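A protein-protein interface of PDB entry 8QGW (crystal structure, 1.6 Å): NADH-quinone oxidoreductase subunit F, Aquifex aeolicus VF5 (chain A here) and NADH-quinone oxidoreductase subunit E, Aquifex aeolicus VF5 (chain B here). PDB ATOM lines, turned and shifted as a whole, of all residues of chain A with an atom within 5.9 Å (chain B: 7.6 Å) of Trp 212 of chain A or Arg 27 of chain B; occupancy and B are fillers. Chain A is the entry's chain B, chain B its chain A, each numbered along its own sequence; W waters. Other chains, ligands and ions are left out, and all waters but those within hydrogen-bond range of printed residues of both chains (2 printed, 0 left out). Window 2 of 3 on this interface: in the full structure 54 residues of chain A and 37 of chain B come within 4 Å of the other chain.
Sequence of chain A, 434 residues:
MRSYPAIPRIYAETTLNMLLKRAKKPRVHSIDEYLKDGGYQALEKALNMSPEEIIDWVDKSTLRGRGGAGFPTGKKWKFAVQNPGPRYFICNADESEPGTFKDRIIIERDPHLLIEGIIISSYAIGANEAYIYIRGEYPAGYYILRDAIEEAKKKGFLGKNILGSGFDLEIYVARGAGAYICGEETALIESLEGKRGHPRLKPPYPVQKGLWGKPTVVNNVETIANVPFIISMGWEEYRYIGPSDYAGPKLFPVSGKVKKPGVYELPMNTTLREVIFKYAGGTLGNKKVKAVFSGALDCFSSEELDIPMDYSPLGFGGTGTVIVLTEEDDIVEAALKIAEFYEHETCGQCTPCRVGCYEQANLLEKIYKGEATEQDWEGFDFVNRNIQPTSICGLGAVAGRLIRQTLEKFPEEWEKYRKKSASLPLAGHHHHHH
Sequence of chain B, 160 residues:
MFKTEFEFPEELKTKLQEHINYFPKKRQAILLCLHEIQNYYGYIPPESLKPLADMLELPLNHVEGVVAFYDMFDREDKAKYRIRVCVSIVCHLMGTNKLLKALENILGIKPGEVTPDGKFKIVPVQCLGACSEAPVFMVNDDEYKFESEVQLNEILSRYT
Hydrophobic or aromatic side chains of chain B within 4 Å of the printed part of chain A: Phe 23, Pro 24, Ile 30 and His 62.
Along chain A the printed residues that touch a printed residue of chain B span positions 129 to 212.
Among the printed residues, 13 pairs touch across the chains.
Among the printed residues, no Asp or Glu carboxylate lies within 4 Å of a Lys or Arg side-chain nitrogen of the other chain.
Water W2 bridges O of Glu 193 of chain A and NE of Arg 27 of chain B.
Water W1 lies within hydrogen-bond range of the indole nitrogen (NE1) of Trp 212 of chain A (2.8 Å), the side-chain amide oxygen (OE1) of Gln 28 of chain B (2.8 Å), the side-chain carboxylate (OE2) of Glu 129 of chain A (2.8 Å) and the side-chain hydroxyl (OH) of Tyr 131 of chain A (3.1 Å).
The side-chain carboxylate of Glu 193 of chain A sits at hydrogen-bond distance from the backbone NH of Trp 212 of chain A, 2.8 Å away.
The side-chain carboxylate of Glu 129 of chain A is in hydrogen-bond range of the side-chain hydroxyl of Tyr 131 of chain A (2.5 Å).
The side-chain carboxylate (OE2) of Glu 193 of chain A is in salt-bridge range of the side-chain amino group (NZ) of Lys 195 of chain A (2.8 Å).
The side-chain amide oxygen of Gln 28 of chain B sits at hydrogen-bond distance from the backbone NH of Lys 25 of chain B (3.2 Å).
The side-chain carboxylate (OE1) of Glu 193 of chain A is in salt-bridge range of the guanidinium group (NH1) of Arg 200 of chain A.
Pro 24 of chain B touches Glu 129 of chain A.
Tyr 131 of chain A touches Phe 23 of chain B.
Pro 24 of chain B touches Tyr 131 of chain A (CD to OH, 3.7 Å).
Arg 27 of chain B touches Glu 193 of chain A (CG to O, 3.7 Å).
Arg 27 of chain B touches Gly 194 of chain A.
Ile 30 of chain B touches Gly 194 of chain A (CG2 to CA, 3.6 Å).
CG of Lys 195 of chain A touches CE1 of His 62 of chain B, 3.9 Å away.
Trp 212 of chain A touches Lys 25 of chain B.
Arg 27 of chain B touches Trp 212 of chain A.
Trp 212 of chain A touches Gln 28 of chain B.
The side-chain amide nitrogen (NE2) of Gln 28 of chain B is in hydrogen-bond range of the backbone carbonyl oxygen (O) of Leu 192 of chain A (3.1 Å).
The side-chain amide nitrogen (NE2) of Gln 28 of chain B sits at hydrogen-bond distance from the side-chain hydroxyl (OH) of Tyr 131 of chain A (3.1 Å).
A ring nitrogen (NE2) of His 62 of chain B sits at hydrogen-bond distance from the backbone carbonyl oxygen (O) of Gly 194 of chain A (2.8 Å).
Printed residues of chain B within 4 Å of Glu 129 of chain A: Pro 24 (3.6 Å).
Printed residues of chain B within 4 Å of Gly 194 of chain A: Arg 27, Ile 30 and His 62.
Trp 212 of chain A touches three residues of chain B.
Of chain A, only Glu 193 (3.7 Å), Gly 194 (3.4 Å) and Trp 212 (3.5 Å) come within 4 Å of Arg 27 of chain B.
Ala 29 of chain B touches none of the printed residues of chain A.
The nearest residue of chain A that does not touch Arg 27 of chain B is Leu 192 of chain A (5.6 Å).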
ATOM      1  N   TYR A  88      17.994 -20.660  28.608  1.00  0.00           N
ATOM      2  CA  TYR A  88      16.883 -20.415  29.516  1.00  0.00           C
ATOM      3  C   TYR A  88      17.142 -21.183  30.800  1.00  0.00           C
ATOM      4  O   TYR A  88      17.719 -22.283  30.777  1.00  0.00           O
ATOM      5  CB  TYR A  88      15.542 -20.836  28.894  1.00  0.00           C
ATOM      6  CG  TYR A  88      15.212 -20.111  27.616  1.00  0.00           C
ATOM      7  CD1 TYR A  88      14.977 -18.752  27.645  1.00  0.00           C
ATOM      8  CD2 TYR A  88      15.191 -20.748  26.388  1.00  0.00           C
ATOM      9  CE1 TYR A  88      14.701 -18.043  26.492  1.00  0.00           C
ATOM     10  CE2 TYR A  88      14.931 -20.051  25.214  1.00  0.00           C
ATOM     11  CZ  TYR A  88      14.664 -18.692  25.276  1.00  0.00           C
ATOM     12  OH  TYR A  88      14.410 -17.988  24.111  1.00  0.00           O
ATOM     13  N   GLU A 129      16.456 -14.926  30.629  1.00  0.00           N
ATOM     14  CA  GLU A 129      15.044 -15.195  30.846  1.00  0.00           C
ATOM     15  C   GLU A 129      14.944 -16.471  31.677  1.00  0.00           C
ATOM     16  O   GLU A 129      15.528 -17.492  31.315  1.00  0.00           O
ATOM     17  CB  GLU A 129      14.374 -15.285  29.476  1.00  0.00           C
ATOM     18  CG  GLU A 129      12.939 -15.783  29.422  1.00  0.00           C
ATOM     19  CD  GLU A 129      12.367 -15.765  28.008  1.00  0.00           C
ATOM     20  OE1 GLU A 129      12.751 -14.856  27.247  1.00  0.00           O
ATOM     21  OE2 GLU A 129      11.510 -16.659  27.666  1.00  0.00           O
ATOM     22  N   TYR A 131      12.179 -18.890  34.308  1.00  0.00           N
ATOM     23  CA  TYR A 131      10.804 -19.194  34.624  1.00  0.00           C
ATOM     24  C   TYR A 131      10.724 -19.932  35.943  1.00  0.00           C
ATOM     25  O   TYR A 131      11.639 -20.663  36.329  1.00  0.00           O
ATOM     26  CB  TYR A 131      10.200 -20.119  33.578  1.00  0.00           C
ATOM     27  CG  TYR A 131      10.038 -19.471  32.253  1.00  0.00           C
ATOM     28  CD1 TYR A 131      11.103 -19.339  31.376  1.00  0.00           C
ATOM     29  CD2 TYR A 131       8.826 -18.908  31.925  1.00  0.00           C
ATOM     30  CE1 TYR A 131      10.937 -18.702  30.161  1.00  0.00           C
ATOM     31  CE2 TYR A 131       8.645 -18.285  30.714  1.00  0.00           C
ATOM     32  CZ  TYR A 131       9.705 -18.152  29.846  1.00  0.00           C
ATOM     33  OH  TYR A 131       9.425 -17.531  28.665  1.00  0.00           O
ATOM     34  N   ILE A 189       8.378 -28.032  29.939  1.00  0.00           N
ATOM     35  CA  ILE A 189       8.701 -27.134  28.829  1.00  0.00           C
ATOM     36  C   ILE A 189       7.575 -27.081  27.791  1.00  0.00           C
ATOM     37  O   ILE A 189       7.226 -26.009  27.334  1.00  0.00           O
ATOM     38  CB  ILE A 189      10.043 -27.573  28.213  1.00  0.00           C
ATOM     39  CG1 ILE A 189      11.174 -27.300  29.205  1.00  0.00           C
ATOM     40  CG2 ILE A 189      10.275 -26.916  26.861  1.00  0.00           C
ATOM     41  CD1 ILE A 189      12.492 -27.915  28.840  1.00  0.00           C
ATOM     42  N   LEU A 192       5.072 -24.749  29.234  1.00  0.00           N
ATOM     43  CA  LEU A 192       5.542 -23.380  29.115  1.00  0.00           C
ATOM     44  C   LEU A 192       5.379 -22.819  27.695  1.00  0.00           C
ATOM     45  O   LEU A 192       5.284 -21.610  27.533  1.00  0.00           O
ATOM     46  CB  LEU A 192       7.013 -23.307  29.518  1.00  0.00           C
ATOM     47  CG  LEU A 192       7.302 -23.233  31.000  1.00  0.00           C
ATOM     48  CD1 LEU A 192       8.803 -23.228  31.243  1.00  0.00           C
ATOM     49  CD2 LEU A 192       6.640 -21.979  31.594  1.00  0.00           C
ATOM     50  N   GLU A 193       5.351 -23.687  26.678  1.00  0.00           N
ATOM     51  CA  GLU A 193       5.234 -23.335  25.279  1.00  0.00           C
ATOM     52  C   GLU A 193       3.750 -23.255  24.878  1.00  0.00           C
ATOM     53  O   GLU A 193       3.425 -23.015  23.714  1.00  0.00           O
ATOM     54  CB  GLU A 193       5.999 -24.354  24.431  1.00  0.00           C
ATOM     55  CG  GLU A 193       7.521 -24.300  24.554  1.00  0.00           C
ATOM     56  CD  GLU A 193       8.277 -25.247  23.620  1.00  0.00           C
ATOM     57  OE1 GLU A 193       9.529 -25.192  23.567  1.00  0.00           O
ATOM     58  OE2 GLU A 193       7.608 -26.052  22.919  1.00  0.00           O
ATOM     59  N   GLY A 194       2.856 -23.459  25.858  1.00  0.00           N
ATOM     60  CA  GLY A 194       1.426 -23.310  25.654  1.00  0.00           C
ATOM     61  C   GLY A 194       0.722 -24.562  25.158  1.00  0.00           C
ATOM     62  O   GLY A 194      -0.384 -24.458  24.622  1.00  0.00           O
ATOM     63  N   LYS A 195       1.348 -25.731  25.341  1.00  0.00           N
ATOM     64  CA  LYS A 195       0.807 -26.984  24.830  1.00  0.00           C
ATOM     65  C   LYS A 195       0.414 -27.924  25.970  1.00  0.00           C
ATOM     66  O   LYS A 195       0.601 -27.643  27.157  1.00  0.00           O
ATOM     67  CB  LYS A 195       1.838 -27.644  23.918  1.00  0.00           C
ATOM     68  CG  LYS A 195       2.085 -26.875  22.622  1.00  0.00           C
ATOM     69  CD  LYS A 195       3.223 -27.416  21.793  1.00  0.00           C
ATOM     70  CE  LYS A 195       4.558 -26.925  22.303  1.00  0.00           C
ATOM     71  NZ  LYS A 195       5.672 -27.516  21.532  1.00  0.00           N
ATOM     72  N   ARG A 200       8.885 -35.344  25.928  1.00  0.00           N
ATOM     73  CA  ARG A 200       9.609 -35.509  24.685  1.00  0.00           C
ATOM     74  C   ARG A 200      10.579 -36.678  24.864  1.00  0.00           C
ATOM     75  O   ARG A 200      11.122 -36.872  25.952  1.00  0.00           O
ATOM     76  CB  ARG A 200      10.427 -34.241  24.367  1.00  0.00           C
ATOM     77  CG  ARG A 200       9.629 -32.938  24.253  1.00  0.00           C
ATOM     78  CD  ARG A 200      10.575 -31.758  24.054  1.00  0.00           C
ATOM     79  NE  ARG A 200       9.950 -30.444  23.906  1.00  0.00           N
ATOM     80  CZ  ARG A 200      10.617 -29.285  23.825  1.00  0.00           C
ATOM     81  NH1 ARG A 200       9.966 -28.150  23.590  1.00  0.00           N
ATOM     82  NH2 ARG A 200      11.941 -29.277  23.912  1.00  0.00           N
ATOM     83  N   GLY A 210      15.773 -27.424  24.511  1.00  0.00           N
ATOM     84  CA  GLY A 210      14.728 -27.234  25.515  1.00  0.00           C
ATOM     85  C   GLY A 210      13.604 -26.297  25.070  1.00  0.00           C
ATOM     86  O   GLY A 210      12.928 -26.531  24.059  1.00  0.00           O
ATOM     87  N   LEU A 211      13.426 -25.217  25.838  1.00  0.00           N
ATOM     88  CA  LEU A 211      12.403 -24.232  25.557  1.00  0.00           C
ATOM     89  C   LEU A 211      12.734 -23.549  24.230  1.00  0.00           C
ATOM     90  O   LEU A 211      13.838 -23.028  24.084  1.00  0.00           O
ATOM     91  CB  LEU A 211      12.356 -23.222  26.704  1.00  0.00           C
ATOM     92  CG  LEU A 211      11.277 -22.143  26.574  1.00  0.00           C
ATOM     93  CD1 LEU A 211       9.887 -22.745  26.665  1.00  0.00           C
ATOM     94  CD2 LEU A 211      11.423 -21.077  27.637  1.00  0.00           C
ATOM     95  N   TRP A 212      11.771 -23.573  23.295  1.00  0.00           N
ATOM     96  CA  TRP A 212      11.935 -23.072  21.938  1.00  0.00           C
ATOM     97  C   TRP A 212      13.155 -23.709  21.265  1.00  0.00           C
ATOM     98  O   TRP A 212      13.764 -23.115  20.371  1.00  0.00           O
ATOM     99  CB  TRP A 212      12.027 -21.537  21.906  1.00  0.00           C
ATOM    100  CG  TRP A 212      10.963 -20.847  22.712  1.00  0.00           C
ATOM    101  CD1 TRP A 212      11.161 -19.932  23.696  1.00  0.00           C
ATOM    102  CD2 TRP A 212       9.536 -21.027  22.613  1.00  0.00           C
ATOM    103  NE1 TRP A 212       9.970 -19.533  24.241  1.00  0.00           N
ATOM    104  CE2 TRP A 212       8.952 -20.182  23.585  1.00  0.00           C
ATOM    105  CE3 TRP A 212       8.697 -21.807  21.811  1.00  0.00           C
ATOM    106  CZ2 TRP A 212       7.572 -20.118  23.788  1.00  0.00           C
ATOM    107  CZ3 TRP A 212       7.331 -21.738  22.009  1.00  0.00           C
ATOM    108  CH2 TRP A 212       6.777 -20.902  22.991  1.00  0.00           C
ATOM    109  N   GLY A 213      13.519 -24.919  21.703  1.00  0.00           N
ATOM    110  CA  GLY A 213      14.612 -25.674  21.123  1.00  0.00           C
ATOM    111  C   GLY A 213      16.003 -25.187  21.542  1.00  0.00           C
ATOM    112  O   GLY A 213      16.985 -25.617  20.947  1.00  0.00           O
ATOM    113  N   LYS A 214      16.079 -24.270  22.511  1.00  0.00           N
ATOM    114  CA  LYS A 214      17.337 -23.664  22.921  1.00  0.00           C
ATOM    115  C   LYS A 214      17.853 -24.365  24.172  1.00  0.00           C
ATOM    116  O   LYS A 214      17.069 -24.956  24.907  1.00  0.00           O
ATOM    117  CB  LYS A 214      17.157 -22.174  23.246  1.00  0.00           C
ATOM    118  CG  LYS A 214      16.537 -21.335  22.141  1.00  0.00           C
ATOM    119  CD  LYS A 214      17.273 -21.371  20.861  1.00  0.00           C
ATOM    120  CE  LYS A 214      16.609 -20.491  19.821  1.00  0.00           C
ATOM    121  NZ  LYS A 214      17.176 -20.746  18.485  1.00  0.00           N
ATOM    122  N   THR A 216      18.450 -25.231  27.780  1.00  0.00           N
ATOM    123  CA  THR A 216      17.614 -24.940  28.923  1.00  0.00           C
ATOM    124  C   THR A 216      18.056 -25.812  30.096  1.00  0.00           C
ATOM    125  O   THR A 216      18.201 -27.037  29.958  1.00  0.00           O
ATOM    126  CB  THR A 216      16.148 -25.217  28.565  1.00  0.00           C
ATOM    127  OG1 THR A 216      15.804 -24.463  27.395  1.00  0.00           O
ATOM    128  CG2 THR A 216      15.173 -24.959  29.691  1.00  0.00           C
ATOM    129  N   ILE B  20      -1.643 -12.115  28.482  1.00  0.00           N
ATOM    130  CA  ILE B  20      -1.140 -12.361  27.135  1.00  0.00           C
ATOM    131  C   ILE B  20       0.118 -11.523  26.892  1.00  0.00           C
ATOM    132  O   ILE B  20       1.049 -11.991  26.240  1.00  0.00           O
ATOM    133  CB  ILE B  20      -2.261 -12.183  26.079  1.00  0.00           C
ATOM    134  CG1 ILE B  20      -3.217 -13.381  26.151  1.00  0.00           C
ATOM    135  CG2 ILE B  20      -1.707 -12.008  24.671  1.00  0.00           C
ATOM    136  CD1 ILE B  20      -4.485 -13.236  25.368  1.00  0.00           C
ATOM    137  N   PHE B  23       4.137 -12.825  29.233  1.00  0.00           N
ATOM    138  CA  PHE B  23       5.217 -13.661  28.747  1.00  0.00           C
ATOM    139  C   PHE B  23       5.756 -13.115  27.427  1.00  0.00           C
ATOM    140  O   PHE B  23       5.115 -12.300  26.745  1.00  0.00           O
ATOM    141  CB  PHE B  23       4.749 -15.102  28.552  1.00  0.00           C
ATOM    142  CG  PHE B  23       4.262 -15.808  29.789  1.00  0.00           C
ATOM    143  CD1 PHE B  23       5.161 -16.322  30.700  1.00  0.00           C
ATOM    144  CD2 PHE B  23       2.910 -15.919  30.059  1.00  0.00           C
ATOM    145  CE1 PHE B  23       4.724 -17.006  31.821  1.00  0.00           C
ATOM    146  CE2 PHE B  23       2.470 -16.585  31.197  1.00  0.00           C
ATOM    147  CZ  PHE B  23       3.381 -17.140  32.067  1.00  0.00           C
ATOM    148  N   PRO B  24       6.971 -13.532  27.010  1.00  0.00           N
ATOM    149  CA  PRO B  24       7.496 -13.099  25.715  1.00  0.00           C
ATOM    150  C   PRO B  24       6.627 -13.471  24.507  1.00  0.00           C
ATOM    151  O   PRO B  24       6.545 -12.674  23.577  1.00  0.00           O
ATOM    152  CB  PRO B  24       8.894 -13.744  25.687  1.00  0.00           C
ATOM    153  CG  PRO B  24       9.253 -13.931  27.147  1.00  0.00           C
ATOM    154  CD  PRO B  24       7.946 -14.298  27.807  1.00  0.00           C
ATOM    155  N   LYS B  25       5.976 -14.653  24.532  1.00  0.00           N
ATOM    156  CA  LYS B  25       5.102 -15.114  23.452  1.00  0.00           C
ATOM    157  C   LYS B  25       3.666 -15.279  23.965  1.00  0.00           C
ATOM    158  O   LYS B  25       3.423 -15.644  25.113  1.00  0.00           O
ATOM    159  CB  LYS B  25       5.625 -16.427  22.848  1.00  0.00           C
ATOM    160  CG  LYS B  25       7.058 -16.365  22.324  1.00  0.00           C
ATOM    161  CD  LYS B  25       7.469 -17.537  21.429  1.00  0.00           C
ATOM    162  CE  LYS B  25       8.901 -17.463  20.933  1.00  0.00           C
ATOM    163  NZ  LYS B  25       9.256 -18.595  20.021  1.00  0.00           N
ATOM    164  N   LYS B  26       2.701 -14.927  23.119  1.00  0.00           N
ATOM    165  CA  LYS B  26       1.317 -14.844  23.553  1.00  0.00           C
ATOM    166  C   LYS B  26       0.815 -16.210  24.008  1.00  0.00           C
ATOM    167  O   LYS B  26       0.109 -16.301  25.004  1.00  0.00           O
ATOM    168  CB  LYS B  26       0.403 -14.371  22.423  1.00  0.00           C
ATOM    169  CG  LYS B  26       0.516 -12.903  22.056  1.00  0.00           C
ATOM    170  CD  LYS B  26      -0.450 -12.509  20.966  1.00  0.00           C
ATOM    171  CE  LYS B  26      -0.528 -11.010  20.779  1.00  0.00           C
ATOM    172  NZ  LYS B  26       0.820 -10.394  20.691  1.00  0.00           N
ATOM    173  N   ARG B  27       1.188 -17.273  23.277  1.00  0.00           N
ATOM    174  CA  ARG B  27       0.609 -18.582  23.528  1.00  0.00           C
ATOM    175  C   ARG B  27       1.037 -19.149  24.875  1.00  0.00           C
ATOM    176  O   ARG B  27       0.393 -20.070  25.368  1.00  0.00           O
ATOM    177  CB  ARG B  27       0.947 -19.568  22.413  1.00  0.00           C
ATOM    178  CG  ARG B  27       2.433 -19.811  22.198  1.00  0.00           C
ATOM    179  CD  ARG B  27       2.578 -20.399  20.814  1.00  0.00           C
ATOM    180  NE  ARG B  27       3.961 -20.655  20.451  1.00  0.00           N
ATOM    181  CZ  ARG B  27       4.696 -19.880  19.657  1.00  0.00           C
ATOM    182  NH1 ARG B  27       5.830 -20.339  19.152  1.00  0.00           N
ATOM    183  NH2 ARG B  27       4.281 -18.670  19.336  1.00  0.00           N
ATOM    184  N   GLN B  28       2.110 -18.616  25.475  1.00  0.00           N
ATOM    185  CA  GLN B  28       2.526 -19.067  26.798  1.00  0.00           C
ATOM    186  C   GLN B  28       1.490 -18.720  27.878  1.00  0.00           C
ATOM    187  O   GLN B  28       1.479 -19.357  28.940  1.00  0.00           O
ATOM    188  CB  GLN B  28       3.901 -18.502  27.175  1.00  0.00           C
ATOM    189  CG  GLN B  28       5.000 -18.771  26.167  1.00  0.00           C
ATOM    190  CD  GLN B  28       6.334 -18.265  26.668  1.00  0.00           C
ATOM    191  OE1 GLN B  28       6.790 -17.183  26.280  1.00  0.00           O
ATOM    192  NE2 GLN B  28       6.970 -19.065  27.515  1.00  0.00           N
ATOM    193  N   ALA B  29       0.579 -17.771  27.596  1.00  0.00           N
ATOM    194  CA  ALA B  29      -0.381 -17.308  28.589  1.00  0.00           C
ATOM    195  C   ALA B  29      -1.631 -18.190  28.673  1.00  0.00           C
ATOM    196  O   ALA B  29      -2.531 -17.905  29.446  1.00  0.00           O
ATOM    197  CB  ALA B  29      -0.743 -15.865  28.315  1.00  0.00           C
ATOM    198  N   ILE B  30      -1.691 -19.288  27.917  1.00  0.00           N
ATOM    199  CA  ILE B  30      -2.931 -20.038  27.753  1.00  0.00           C
ATOM    200  C   ILE B  30      -3.509 -20.520  29.083  1.00  0.00           C
ATOM    201  O   ILE B  30      -4.712 -20.417  29.280  1.00  0.00           O
ATOM    202  CB  ILE B  30      -2.742 -21.208  26.769  1.00  0.00           C
ATOM    203  CG1 ILE B  30      -4.069 -21.922  26.501  1.00  0.00           C
ATOM    204  CG2 ILE B  30      -1.658 -22.176  27.239  1.00  0.00           C
ATOM    205  CD1 ILE B  30      -4.057 -22.765  25.247  1.00  0.00           C
ATOM    206  N   LEU B  31      -2.688 -21.100  29.965  1.00  0.00           N
ATOM    207  CA  LEU B  31      -3.204 -21.611  31.236  1.00  0.00           C
ATOM    208  C   LEU B  31      -3.627 -20.488  32.185  1.00  0.00           C
ATOM    209  O   LEU B  31      -4.632 -20.641  32.885  1.00  0.00           O
ATOM    210  CB  LEU B  31      -2.165 -22.511  31.912  1.00  0.00           C
ATOM    211  CG  LEU B  31      -1.746 -23.718  31.076  1.00  0.00           C
ATOM    212  CD1 LEU B  31      -0.836 -24.645  31.846  1.00  0.00           C
ATOM    213  CD2 LEU B  31      -2.953 -24.486  30.554  1.00  0.00           C
ATOM    214  N   MET B  55      -7.398 -14.513  20.643  1.00  0.00           N
ATOM    215  CA  MET B  55      -6.542 -13.619  21.418  1.00  0.00           C
ATOM    216  C   MET B  55      -5.126 -14.188  21.557  1.00  0.00           C
ATOM    217  O   MET B  55      -4.164 -13.423  21.577  1.00  0.00           O
ATOM    218  CB  MET B  55      -7.118 -13.388  22.820  1.00  0.00           C
ATOM    219  CG  MET B  55      -8.367 -12.519  22.834  1.00  0.00           C
ATOM    220  SD  MET B  55      -9.043 -12.353  24.510  1.00  0.00           S
ATOM    221  CE  MET B  55      -7.839 -11.232  25.225  1.00  0.00           C
ATOM    222  N   LEU B  56      -5.012 -15.521  21.654  1.00  0.00           N
ATOM    223  CA  LEU B  56      -3.727 -16.203  21.778  1.00  0.00           C
ATOM    224  C   LEU B  56      -3.080 -16.445  20.405  1.00  0.00           C
ATOM    225  O   LEU B  56      -1.940 -16.903  20.333  1.00  0.00           O
ATOM    226  CB  LEU B  56      -3.950 -17.541  22.497  1.00  0.00           C
ATOM    227  CG  LEU B  56      -4.381 -17.506  23.967  1.00  0.00           C
ATOM    228  CD1 LEU B  56      -4.878 -18.869  24.410  1.00  0.00           C
ATOM    229  CD2 LEU B  56      -3.244 -17.068  24.874  1.00  0.00           C
ATOM    230  N   GLU B  57      -3.827 -16.203  19.319  1.00  0.00           N
ATOM    231  CA  GLU B  57      -3.390 -16.484  17.949  1.00  0.00           C
ATOM    232  C   GLU B  57      -3.064 -17.973  17.812  1.00  0.00           C
ATOM    233  O   GLU B  57      -2.041 -18.345  17.244  1.00  0.00           O
ATOM    234  CB  GLU B  57      -2.219 -15.577  17.543  1.00  0.00           C
ATOM    235  CG  GLU B  57      -2.600 -14.102  17.445  1.00  0.00           C
ATOM    236  CD  GLU B  57      -1.452 -13.109  17.306  1.00  0.00           C
ATOM    237  OE1 GLU B  57      -1.736 -11.909  17.194  1.00  0.00           O
ATOM    238  OE2 GLU B  57      -0.273 -13.522  17.345  1.00  0.00           O
ATOM    239  N   LEU B  58      -3.953 -18.809  18.367  1.00  0.00           N
ATOM    240  CA  LEU B  58      -3.864 -20.260  18.315  1.00  0.00           C
ATOM    241  C   LEU B  58      -5.103 -20.816  17.615  1.00  0.00           C
ATOM    242  O   LEU B  58      -6.184 -20.235  17.663  1.00  0.00           O
ATOM    243  CB  LEU B  58      -3.777 -20.815  19.743  1.00  0.00           C
ATOM    244  CG  LEU B  58      -2.427 -20.675  20.445  1.00  0.00           C
ATOM    245  CD1 LEU B  58      -2.487 -21.256  21.844  1.00  0.00           C
ATOM    246  CD2 LEU B  58      -1.310 -21.308  19.639  1.00  0.00           C
ATOM    247  N   HIS B  62      -6.449 -26.487  19.189  1.00  0.00           N
ATOM    248  CA  HIS B  62      -5.341 -26.425  20.139  1.00  0.00           C
ATOM    249  C   HIS B  62      -5.859 -26.052  21.526  1.00  0.00           C
ATOM    250  O   HIS B  62      -5.530 -26.702  22.513  1.00  0.00           O
ATOM    251  CB  HIS B  62      -4.271 -25.428  19.676  1.00  0.00           C
ATOM    252  CG  HIS B  62      -3.080 -25.299  20.574  1.00  0.00           C
ATOM    253  ND1 HIS B  62      -1.810 -25.191  20.055  1.00  0.00           N
ATOM    254  CD2 HIS B  62      -2.954 -25.195  21.909  1.00  0.00           C
ATOM    255  CE1 HIS B  62      -0.953 -25.071  21.064  1.00  0.00           C
ATOM    256  NE2 HIS B  62      -1.626 -25.069  22.195  1.00  0.00           N
HETATM  257  O   HOH W   1       9.556 -17.111  25.642  1.00  0.00           O
HETATM  258  O   HOH W   2       4.048 -23.445  21.129  1.00  0.00           O
